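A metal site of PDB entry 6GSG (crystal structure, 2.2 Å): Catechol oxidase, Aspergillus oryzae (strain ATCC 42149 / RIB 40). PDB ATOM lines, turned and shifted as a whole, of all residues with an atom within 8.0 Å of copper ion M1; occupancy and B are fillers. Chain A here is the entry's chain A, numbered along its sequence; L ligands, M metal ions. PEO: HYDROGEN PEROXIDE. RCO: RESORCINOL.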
ATOM      1  N   HIS A 102     -26.162  -2.414   1.868  1.00  0.00           N
ATOM      2  CA  HIS A 102     -25.417  -3.442   1.138  1.00  0.00           C
ATOM      3  C   HIS A 102     -24.688  -4.373   2.100  1.00  0.00           C
ATOM      4  O   HIS A 102     -24.681  -5.594   1.915  1.00  0.00           O
ATOM      5  CB  HIS A 102     -24.432  -2.778   0.169  1.00  0.00           C
ATOM      6  CG  HIS A 102     -23.777  -3.737  -0.773  1.00  0.00           C
ATOM      7  ND1 HIS A 102     -22.681  -4.493  -0.408  1.00  0.00           N
ATOM      8  CD2 HIS A 102     -24.070  -4.091  -2.039  1.00  0.00           C
ATOM      9  CE1 HIS A 102     -22.313  -5.245  -1.430  1.00  0.00           C
ATOM     10  NE2 HIS A 102     -23.147  -5.036  -2.426  1.00  0.00           N
ATOM     11  N   ILE A 103     -24.050  -3.807   3.138  1.00  0.00           N
ATOM     12  CA  ILE A 103     -23.464  -4.633   4.185  1.00  0.00           C
ATOM     13  C   ILE A 103     -24.519  -5.555   4.780  1.00  0.00           C
ATOM     14  O   ILE A 103     -24.275  -6.739   5.019  1.00  0.00           O
ATOM     15  CB  ILE A 103     -22.842  -3.740   5.278  1.00  0.00           C
ATOM     16  CG1 ILE A 103     -21.641  -2.952   4.743  1.00  0.00           C
ATOM     17  CG2 ILE A 103     -22.433  -4.585   6.492  1.00  0.00           C
ATOM     18  CD1 ILE A 103     -21.229  -1.819   5.656  1.00  0.00           C
ATOM     19  N   GLN A 105     -27.327  -6.770   3.638  1.00  0.00           N
ATOM     20  CA  GLN A 105     -27.990  -7.757   2.783  1.00  0.00           C
ATOM     21  C   GLN A 105     -27.033  -8.573   1.927  1.00  0.00           C
ATOM     22  O   GLN A 105     -27.496  -9.372   1.109  1.00  0.00           O
ATOM     23  CB  GLN A 105     -29.023  -7.062   1.883  1.00  0.00           C
ATOM     24  CG  GLN A 105     -30.069  -6.251   2.642  1.00  0.00           C
ATOM     25  CD  GLN A 105     -31.238  -5.860   1.767  1.00  0.00           C
ATOM     26  OE1 GLN A 105     -31.961  -6.717   1.249  1.00  0.00           O
ATOM     27  NE2 GLN A 105     -31.442  -4.558   1.590  1.00  0.00           N
ATOM     28  N   THR A 106     -25.714  -8.403   2.112  1.00  0.00           N
ATOM     29  CA  THR A 106     -24.732  -9.059   1.249  1.00  0.00           C
ATOM     30  C   THR A 106     -24.977 -10.571   1.141  1.00  0.00           C
ATOM     31  O   THR A 106     -24.788 -11.156   0.069  1.00  0.00           O
ATOM     32  CB  THR A 106     -23.326  -8.780   1.788  1.00  0.00           C
ATOM     33  OG1 THR A 106     -22.909  -7.468   1.372  1.00  0.00           O
ATOM     34  CG2 THR A 106     -22.322  -9.811   1.279  1.00  0.00           C
ATOM     35  N   ILE A 109     -27.888 -11.118  -1.542  1.00  0.00           N
ATOM     36  CA  ILE A 109     -27.886 -10.384  -2.810  1.00  0.00           C
ATOM     37  C   ILE A 109     -26.722 -10.758  -3.704  1.00  0.00           C
ATOM     38  O   ILE A 109     -26.562 -10.160  -4.778  1.00  0.00           O
ATOM     39  CB  ILE A 109     -27.913  -8.855  -2.581  1.00  0.00           C
ATOM     40  CG1 ILE A 109     -26.669  -8.409  -1.813  1.00  0.00           C
ATOM     41  CG2 ILE A 109     -29.183  -8.432  -1.865  1.00  0.00           C
ATOM     42  CD1 ILE A 109     -26.582  -6.924  -1.592  1.00  0.00           C
ATOM     43  N   HIS A 110     -25.884 -11.725  -3.312  1.00  0.00           N
ATOM     44  CA  HIS A 110     -24.807 -12.217  -4.143  1.00  0.00           C
ATOM     45  C   HIS A 110     -24.937 -13.728  -4.272  1.00  0.00           C
ATOM     46  O   HIS A 110     -25.265 -14.414  -3.298  1.00  0.00           O
ATOM     47  CB  HIS A 110     -23.429 -11.838  -3.555  1.00  0.00           C
ATOM     48  CG  HIS A 110     -23.215 -10.362  -3.445  1.00  0.00           C
ATOM     49  ND1 HIS A 110     -23.366  -9.673  -2.247  1.00  0.00           N
ATOM     50  CD2 HIS A 110     -22.883  -9.427  -4.372  1.00  0.00           C
ATOM     51  CE1 HIS A 110     -23.117  -8.388  -2.448  1.00  0.00           C
ATOM     52  NE2 HIS A 110     -22.830  -8.214  -3.731  1.00  0.00           N
ATOM     53  N   PHE A 115     -29.433 -11.420  -7.582  1.00  0.00           N
ATOM     54  CA  PHE A 115     -28.191 -10.658  -7.685  1.00  0.00           C
ATOM     55  C   PHE A 115     -28.296  -9.532  -8.723  1.00  0.00           C
ATOM     56  O   PHE A 115     -28.054  -8.359  -8.411  1.00  0.00           O
ATOM     57  CB  PHE A 115     -27.026 -11.587  -8.013  1.00  0.00           C
ATOM     58  CG  PHE A 115     -25.795 -10.884  -8.508  1.00  0.00           C
ATOM     59  CD1 PHE A 115     -25.052 -10.079  -7.656  1.00  0.00           C
ATOM     60  CD2 PHE A 115     -25.374 -11.012  -9.828  1.00  0.00           C
ATOM     61  CE1 PHE A 115     -23.906  -9.420  -8.104  1.00  0.00           C
ATOM     62  CE2 PHE A 115     -24.234 -10.362 -10.284  1.00  0.00           C
ATOM     63  CZ  PHE A 115     -23.504  -9.562  -9.418  1.00  0.00           C
ATOM     64  N   TRP A 118     -31.455  -6.987  -8.030  1.00  0.00           N
ATOM     65  CA  TRP A 118     -31.211  -6.171  -6.849  1.00  0.00           C
ATOM     66  C   TRP A 118     -30.207  -5.056  -7.159  1.00  0.00           C
ATOM     67  O   TRP A 118     -30.410  -3.908  -6.759  1.00  0.00           O
ATOM     68  CB  TRP A 118     -30.694  -7.039  -5.696  1.00  0.00           C
ATOM     69  CG  TRP A 118     -30.631  -6.319  -4.376  1.00  0.00           C
ATOM     70  CD1 TRP A 118     -31.549  -6.371  -3.376  1.00  0.00           C
ATOM     71  CD2 TRP A 118     -29.571  -5.470  -3.918  1.00  0.00           C
ATOM     72  NE1 TRP A 118     -31.131  -5.597  -2.314  1.00  0.00           N
ATOM     73  CE2 TRP A 118     -29.929  -5.029  -2.616  1.00  0.00           C
ATOM     74  CE3 TRP A 118     -28.357  -5.029  -4.461  1.00  0.00           C
ATOM     75  CZ2 TRP A 118     -29.119  -4.174  -1.867  1.00  0.00           C
ATOM     76  CZ3 TRP A 118     -27.554  -4.172  -3.719  1.00  0.00           C
ATOM     77  CH2 TRP A 118     -27.936  -3.763  -2.436  1.00  0.00           C
ATOM     78  N   HIS A 119     -29.130  -5.387  -7.866  1.00  0.00           N
ATOM     79  CA  HIS A 119     -28.116  -4.369  -8.145  1.00  0.00           C
ATOM     80  C   HIS A 119     -28.600  -3.375  -9.182  1.00  0.00           C
ATOM     81  O   HIS A 119     -28.195  -2.203  -9.155  1.00  0.00           O
ATOM     82  CB  HIS A 119     -26.808  -5.041  -8.563  1.00  0.00           C
ATOM     83  CG  HIS A 119     -26.045  -5.613  -7.407  1.00  0.00           C
ATOM     84  ND1 HIS A 119     -26.326  -6.855  -6.872  1.00  0.00           N
ATOM     85  CD2 HIS A 119     -25.041  -5.108  -6.657  1.00  0.00           C
ATOM     86  CE1 HIS A 119     -25.508  -7.091  -5.858  1.00  0.00           C
ATOM     87  NE2 HIS A 119     -24.720  -6.049  -5.707  1.00  0.00           N
ATOM     88  N   PHE A 122     -30.552  -1.158  -7.014  1.00  0.00           N
ATOM     89  CA  PHE A 122     -29.630  -0.433  -6.138  1.00  0.00           C
ATOM     90  C   PHE A 122     -29.075   0.817  -6.812  1.00  0.00           C
ATOM     91  O   PHE A 122     -29.152   1.926  -6.269  1.00  0.00           O
ATOM     92  CB  PHE A 122     -28.495  -1.370  -5.715  1.00  0.00           C
ATOM     93  CG  PHE A 122     -27.691  -0.875  -4.550  1.00  0.00           C
ATOM     94  CD1 PHE A 122     -28.306  -0.381  -3.410  1.00  0.00           C
ATOM     95  CD2 PHE A 122     -26.302  -0.953  -4.567  1.00  0.00           C
ATOM     96  CE1 PHE A 122     -27.561   0.059  -2.330  1.00  0.00           C
ATOM     97  CE2 PHE A 122     -25.547  -0.529  -3.499  1.00  0.00           C
ATOM     98  CZ  PHE A 122     -26.180  -0.016  -2.368  1.00  0.00           C
ATOM     99  N   HIS A 284     -17.251  -9.493 -12.862  1.00  0.00           N
ATOM    100  CA  HIS A 284     -17.711  -8.837 -11.636  1.00  0.00           C
ATOM    101  C   HIS A 284     -16.602  -8.786 -10.595  1.00  0.00           C
ATOM    102  O   HIS A 284     -16.197  -7.706 -10.152  1.00  0.00           O
ATOM    103  CB  HIS A 284     -18.937  -9.560 -11.087  1.00  0.00           C
ATOM    104  CG  HIS A 284     -19.474  -8.952  -9.836  1.00  0.00           C
ATOM    105  ND1 HIS A 284     -19.508  -9.637  -8.635  1.00  0.00           N
ATOM    106  CD2 HIS A 284     -19.995  -7.731  -9.589  1.00  0.00           C
ATOM    107  CE1 HIS A 284     -20.034  -8.860  -7.707  1.00  0.00           C
ATOM    108  NE2 HIS A 284     -20.336  -7.696  -8.256  1.00  0.00           N
ATOM    109  N   HIS A 288     -14.041  -5.560  -9.385  1.00  0.00           N
ATOM    110  CA  HIS A 288     -13.977  -5.179  -7.971  1.00  0.00           C
ATOM    111  C   HIS A 288     -12.539  -5.229  -7.460  1.00  0.00           C
ATOM    112  O   HIS A 288     -11.993  -4.224  -6.997  1.00  0.00           O
ATOM    113  CB  HIS A 288     -14.865  -6.109  -7.143  1.00  0.00           C
ATOM    114  CG  HIS A 288     -16.284  -5.647  -7.009  1.00  0.00           C
ATOM    115  ND1 HIS A 288     -16.626  -4.444  -6.424  1.00  0.00           N
ATOM    116  CD2 HIS A 288     -17.450  -6.222  -7.373  1.00  0.00           C
ATOM    117  CE1 HIS A 288     -17.932  -4.306  -6.437  1.00  0.00           C
ATOM    118  NE2 HIS A 288     -18.459  -5.368  -7.012  1.00  0.00           N
ATOM    119  N   VAL A 299     -16.315  -7.520   0.233  1.00  0.00           N
ATOM    120  CA  VAL A 299     -17.564  -7.792  -0.480  1.00  0.00           C
ATOM    121  C   VAL A 299     -18.721  -7.027   0.162  1.00  0.00           C
ATOM    122  O   VAL A 299     -19.626  -6.546  -0.541  1.00  0.00           O
ATOM    123  CB  VAL A 299     -17.819  -9.309  -0.517  1.00  0.00           C
ATOM    124  CG1 VAL A 299     -19.188  -9.610  -1.126  1.00  0.00           C
ATOM    125  CG2 VAL A 299     -16.733 -10.019  -1.288  1.00  0.00           C
ATOM    126  N   TYR A 300     -18.698  -6.892   1.483  1.00  0.00           N
ATOM    127  CA  TYR A 300     -19.816  -6.266   2.183  1.00  0.00           C
ATOM    128  C   TYR A 300     -19.827  -4.753   1.977  1.00  0.00           C
ATOM    129  O   TYR A 300     -20.897  -4.161   1.788  1.00  0.00           O
ATOM    130  CB  TYR A 300     -19.745  -6.570   3.679  1.00  0.00           C
ATOM    131  CG  TYR A 300     -20.006  -8.007   4.069  1.00  0.00           C
ATOM    132  CD1 TYR A 300     -19.036  -8.984   3.882  1.00  0.00           C
ATOM    133  CD2 TYR A 300     -21.216  -8.381   4.639  1.00  0.00           C
ATOM    134  CE1 TYR A 300     -19.274 -10.300   4.250  1.00  0.00           C
ATOM    135  CE2 TYR A 300     -21.464  -9.688   5.002  1.00  0.00           C
ATOM    136  CZ  TYR A 300     -20.484 -10.640   4.804  1.00  0.00           C
ATOM    137  OH  TYR A 300     -20.731 -11.946   5.167  1.00  0.00           O
ATOM    138  N   VAL A 301     -18.652  -4.128   1.989  1.00  0.00           N
ATOM    139  CA  VAL A 301     -18.521  -2.677   2.057  1.00  0.00           C
ATOM    140  C   VAL A 301     -18.165  -2.067   0.707  1.00  0.00           C
ATOM    141  O   VAL A 301     -17.935  -0.858   0.615  1.00  0.00           O
ATOM    142  CB  VAL A 301     -17.494  -2.295   3.136  1.00  0.00           C
ATOM    143  CG1 VAL A 301     -17.625  -0.833   3.569  1.00  0.00           C
ATOM    144  CG2 VAL A 301     -17.648  -3.207   4.345  1.00  0.00           C
ATOM    145  N   SER A 302     -18.141  -2.872  -0.368  1.00  0.00           N
ATOM    146  CA  SER A 302     -17.665  -2.409  -1.660  1.00  0.00           C
ATOM    147  C   SER A 302     -18.308  -1.121  -2.171  1.00  0.00           C
ATOM    148  O   SER A 302     -17.600  -0.319  -2.802  1.00  0.00           O
ATOM    149  CB  SER A 302     -17.828  -3.517  -2.714  1.00  0.00           C
ATOM    150  OG  SER A 302     -19.165  -3.991  -2.782  1.00  0.00           O
ATOM    151  N   PRO A 303     -19.602  -0.833  -1.940  1.00  0.00           N
ATOM    152  CA  PRO A 303     -20.118   0.487  -2.353  1.00  0.00           C
ATOM    153  C   PRO A 303     -19.395   1.673  -1.724  1.00  0.00           C
ATOM    154  O   PRO A 303     -19.538   2.798  -2.211  1.00  0.00           O
ATOM    155  CB  PRO A 303     -21.596   0.450  -1.926  1.00  0.00           C
ATOM    156  CG  PRO A 303     -21.928  -0.992  -1.936  1.00  0.00           C
ATOM    157  CD  PRO A 303     -20.702  -1.673  -1.428  1.00  0.00           C
ATOM    158  N   PHE A 308     -17.613   1.914  -7.451  1.00  0.00           N
ATOM    159  CA  PHE A 308     -18.639   0.872  -7.428  1.00  0.00           C
ATOM    160  C   PHE A 308     -19.791   1.189  -8.384  1.00  0.00           C
ATOM    161  O   PHE A 308     -20.287   0.303  -9.094  1.00  0.00           O
ATOM    162  CB  PHE A 308     -19.164   0.695  -6.001  1.00  0.00           C
ATOM    163  CG  PHE A 308     -20.339  -0.247  -5.870  1.00  0.00           C
ATOM    164  CD1 PHE A 308     -21.632   0.204  -6.100  1.00  0.00           C
ATOM    165  CD2 PHE A 308     -20.148  -1.561  -5.487  1.00  0.00           C
ATOM    166  CE1 PHE A 308     -22.706  -0.659  -5.976  1.00  0.00           C
ATOM    167  CE2 PHE A 308     -21.214  -2.424  -5.356  1.00  0.00           C
ATOM    168  CZ  PHE A 308     -22.501  -1.968  -5.606  1.00  0.00           C
ATOM    169  N   HIS A 312     -20.873  -1.143 -11.596  1.00  0.00           N
ATOM    170  CA  HIS A 312     -22.145  -1.848 -11.697  1.00  0.00           C
ATOM    171  C   HIS A 312     -23.064  -1.268 -12.755  1.00  0.00           C
ATOM    172  O   HIS A 312     -23.991  -1.956 -13.192  1.00  0.00           O
ATOM    173  CB  HIS A 312     -22.840  -1.875 -10.331  1.00  0.00           C
ATOM    174  CG  HIS A 312     -22.507  -3.093  -9.535  1.00  0.00           C
ATOM    175  ND1 HIS A 312     -23.155  -4.294  -9.710  1.00  0.00           N
ATOM    176  CD2 HIS A 312     -21.550  -3.313  -8.600  1.00  0.00           C
ATOM    177  CE1 HIS A 312     -22.645  -5.190  -8.894  1.00  0.00           C
ATOM    178  NE2 HIS A 312     -21.668  -4.623  -8.217  1.00  0.00           N
HETATM  179  O1  PEO L   1     -20.296  -6.277  -4.224  1.00  0.00           O
HETATM  180  O2  PEO L   1     -21.300  -6.179  -5.259  1.00  0.00           O
HETATM  181  C1  RCO L   2     -18.130  -8.527  -4.689  1.00  0.00           C
HETATM  182  C2  RCO L   2     -17.524  -7.422  -4.111  1.00  0.00           C
HETATM  183  C3  RCO L   2     -16.138  -7.338  -4.062  1.00  0.00           C
HETATM  184  C4  RCO L   2     -15.357  -8.362  -4.577  1.00  0.00           C
HETATM  185  C5  RCO L   2     -15.977  -9.469  -5.155  1.00  0.00           C
HETATM  186  C6  RCO L   2     -17.355  -9.560  -5.213  1.00  0.00           C
HETATM  187  O1  RCO L   2     -19.488  -8.606  -4.740  1.00  0.00           O
HETATM  188  O3  RCO L   2     -15.545  -6.245  -3.485  1.00  0.00           O
HETATM  189 CU    CU M   1     -23.384  -6.047  -4.127  1.00  0.00          CU
HETATM  190 CU    CU M   2     -20.407  -5.875  -7.299  1.00  0.00          CU
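Copper ion M1 is bound by NE2 of His 102 (2.0 Å), NE2 of His 119 (2.1 Å), NE2 of His 110 (2.3 Å) and O2 of PEO L1 (2.4 Å). Copper ion M1 has four donor atoms within binding distance.
The backbone carbonyl oxygen (O) of His 102 sits at hydrogen-bond distance from the side-chain hydroxyl (OG1) of Thr 106. A ring nitrogen (ND1) of His 102 lies within hydrogen-bond range of the backbone carbonyl oxygen (O) of Tyr 300, 2.8 Å away. A ring nitrogen (ND1) of His 119 lies within hydrogen-bond range of the backbone carbonyl oxygen of Phe 115 (2.8 Å). A ring nitrogen (ND1) of His 110 is in hydrogen-bond range of the backbone carbonyl oxygen (O) of Thr 106 (3.1 Å).
Of the 19 residues printed, 3 come within 4 Å of copper ion M1. The nearest printed residue that does not touch copper ion M1 is Ile 109 (4.2 Å).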
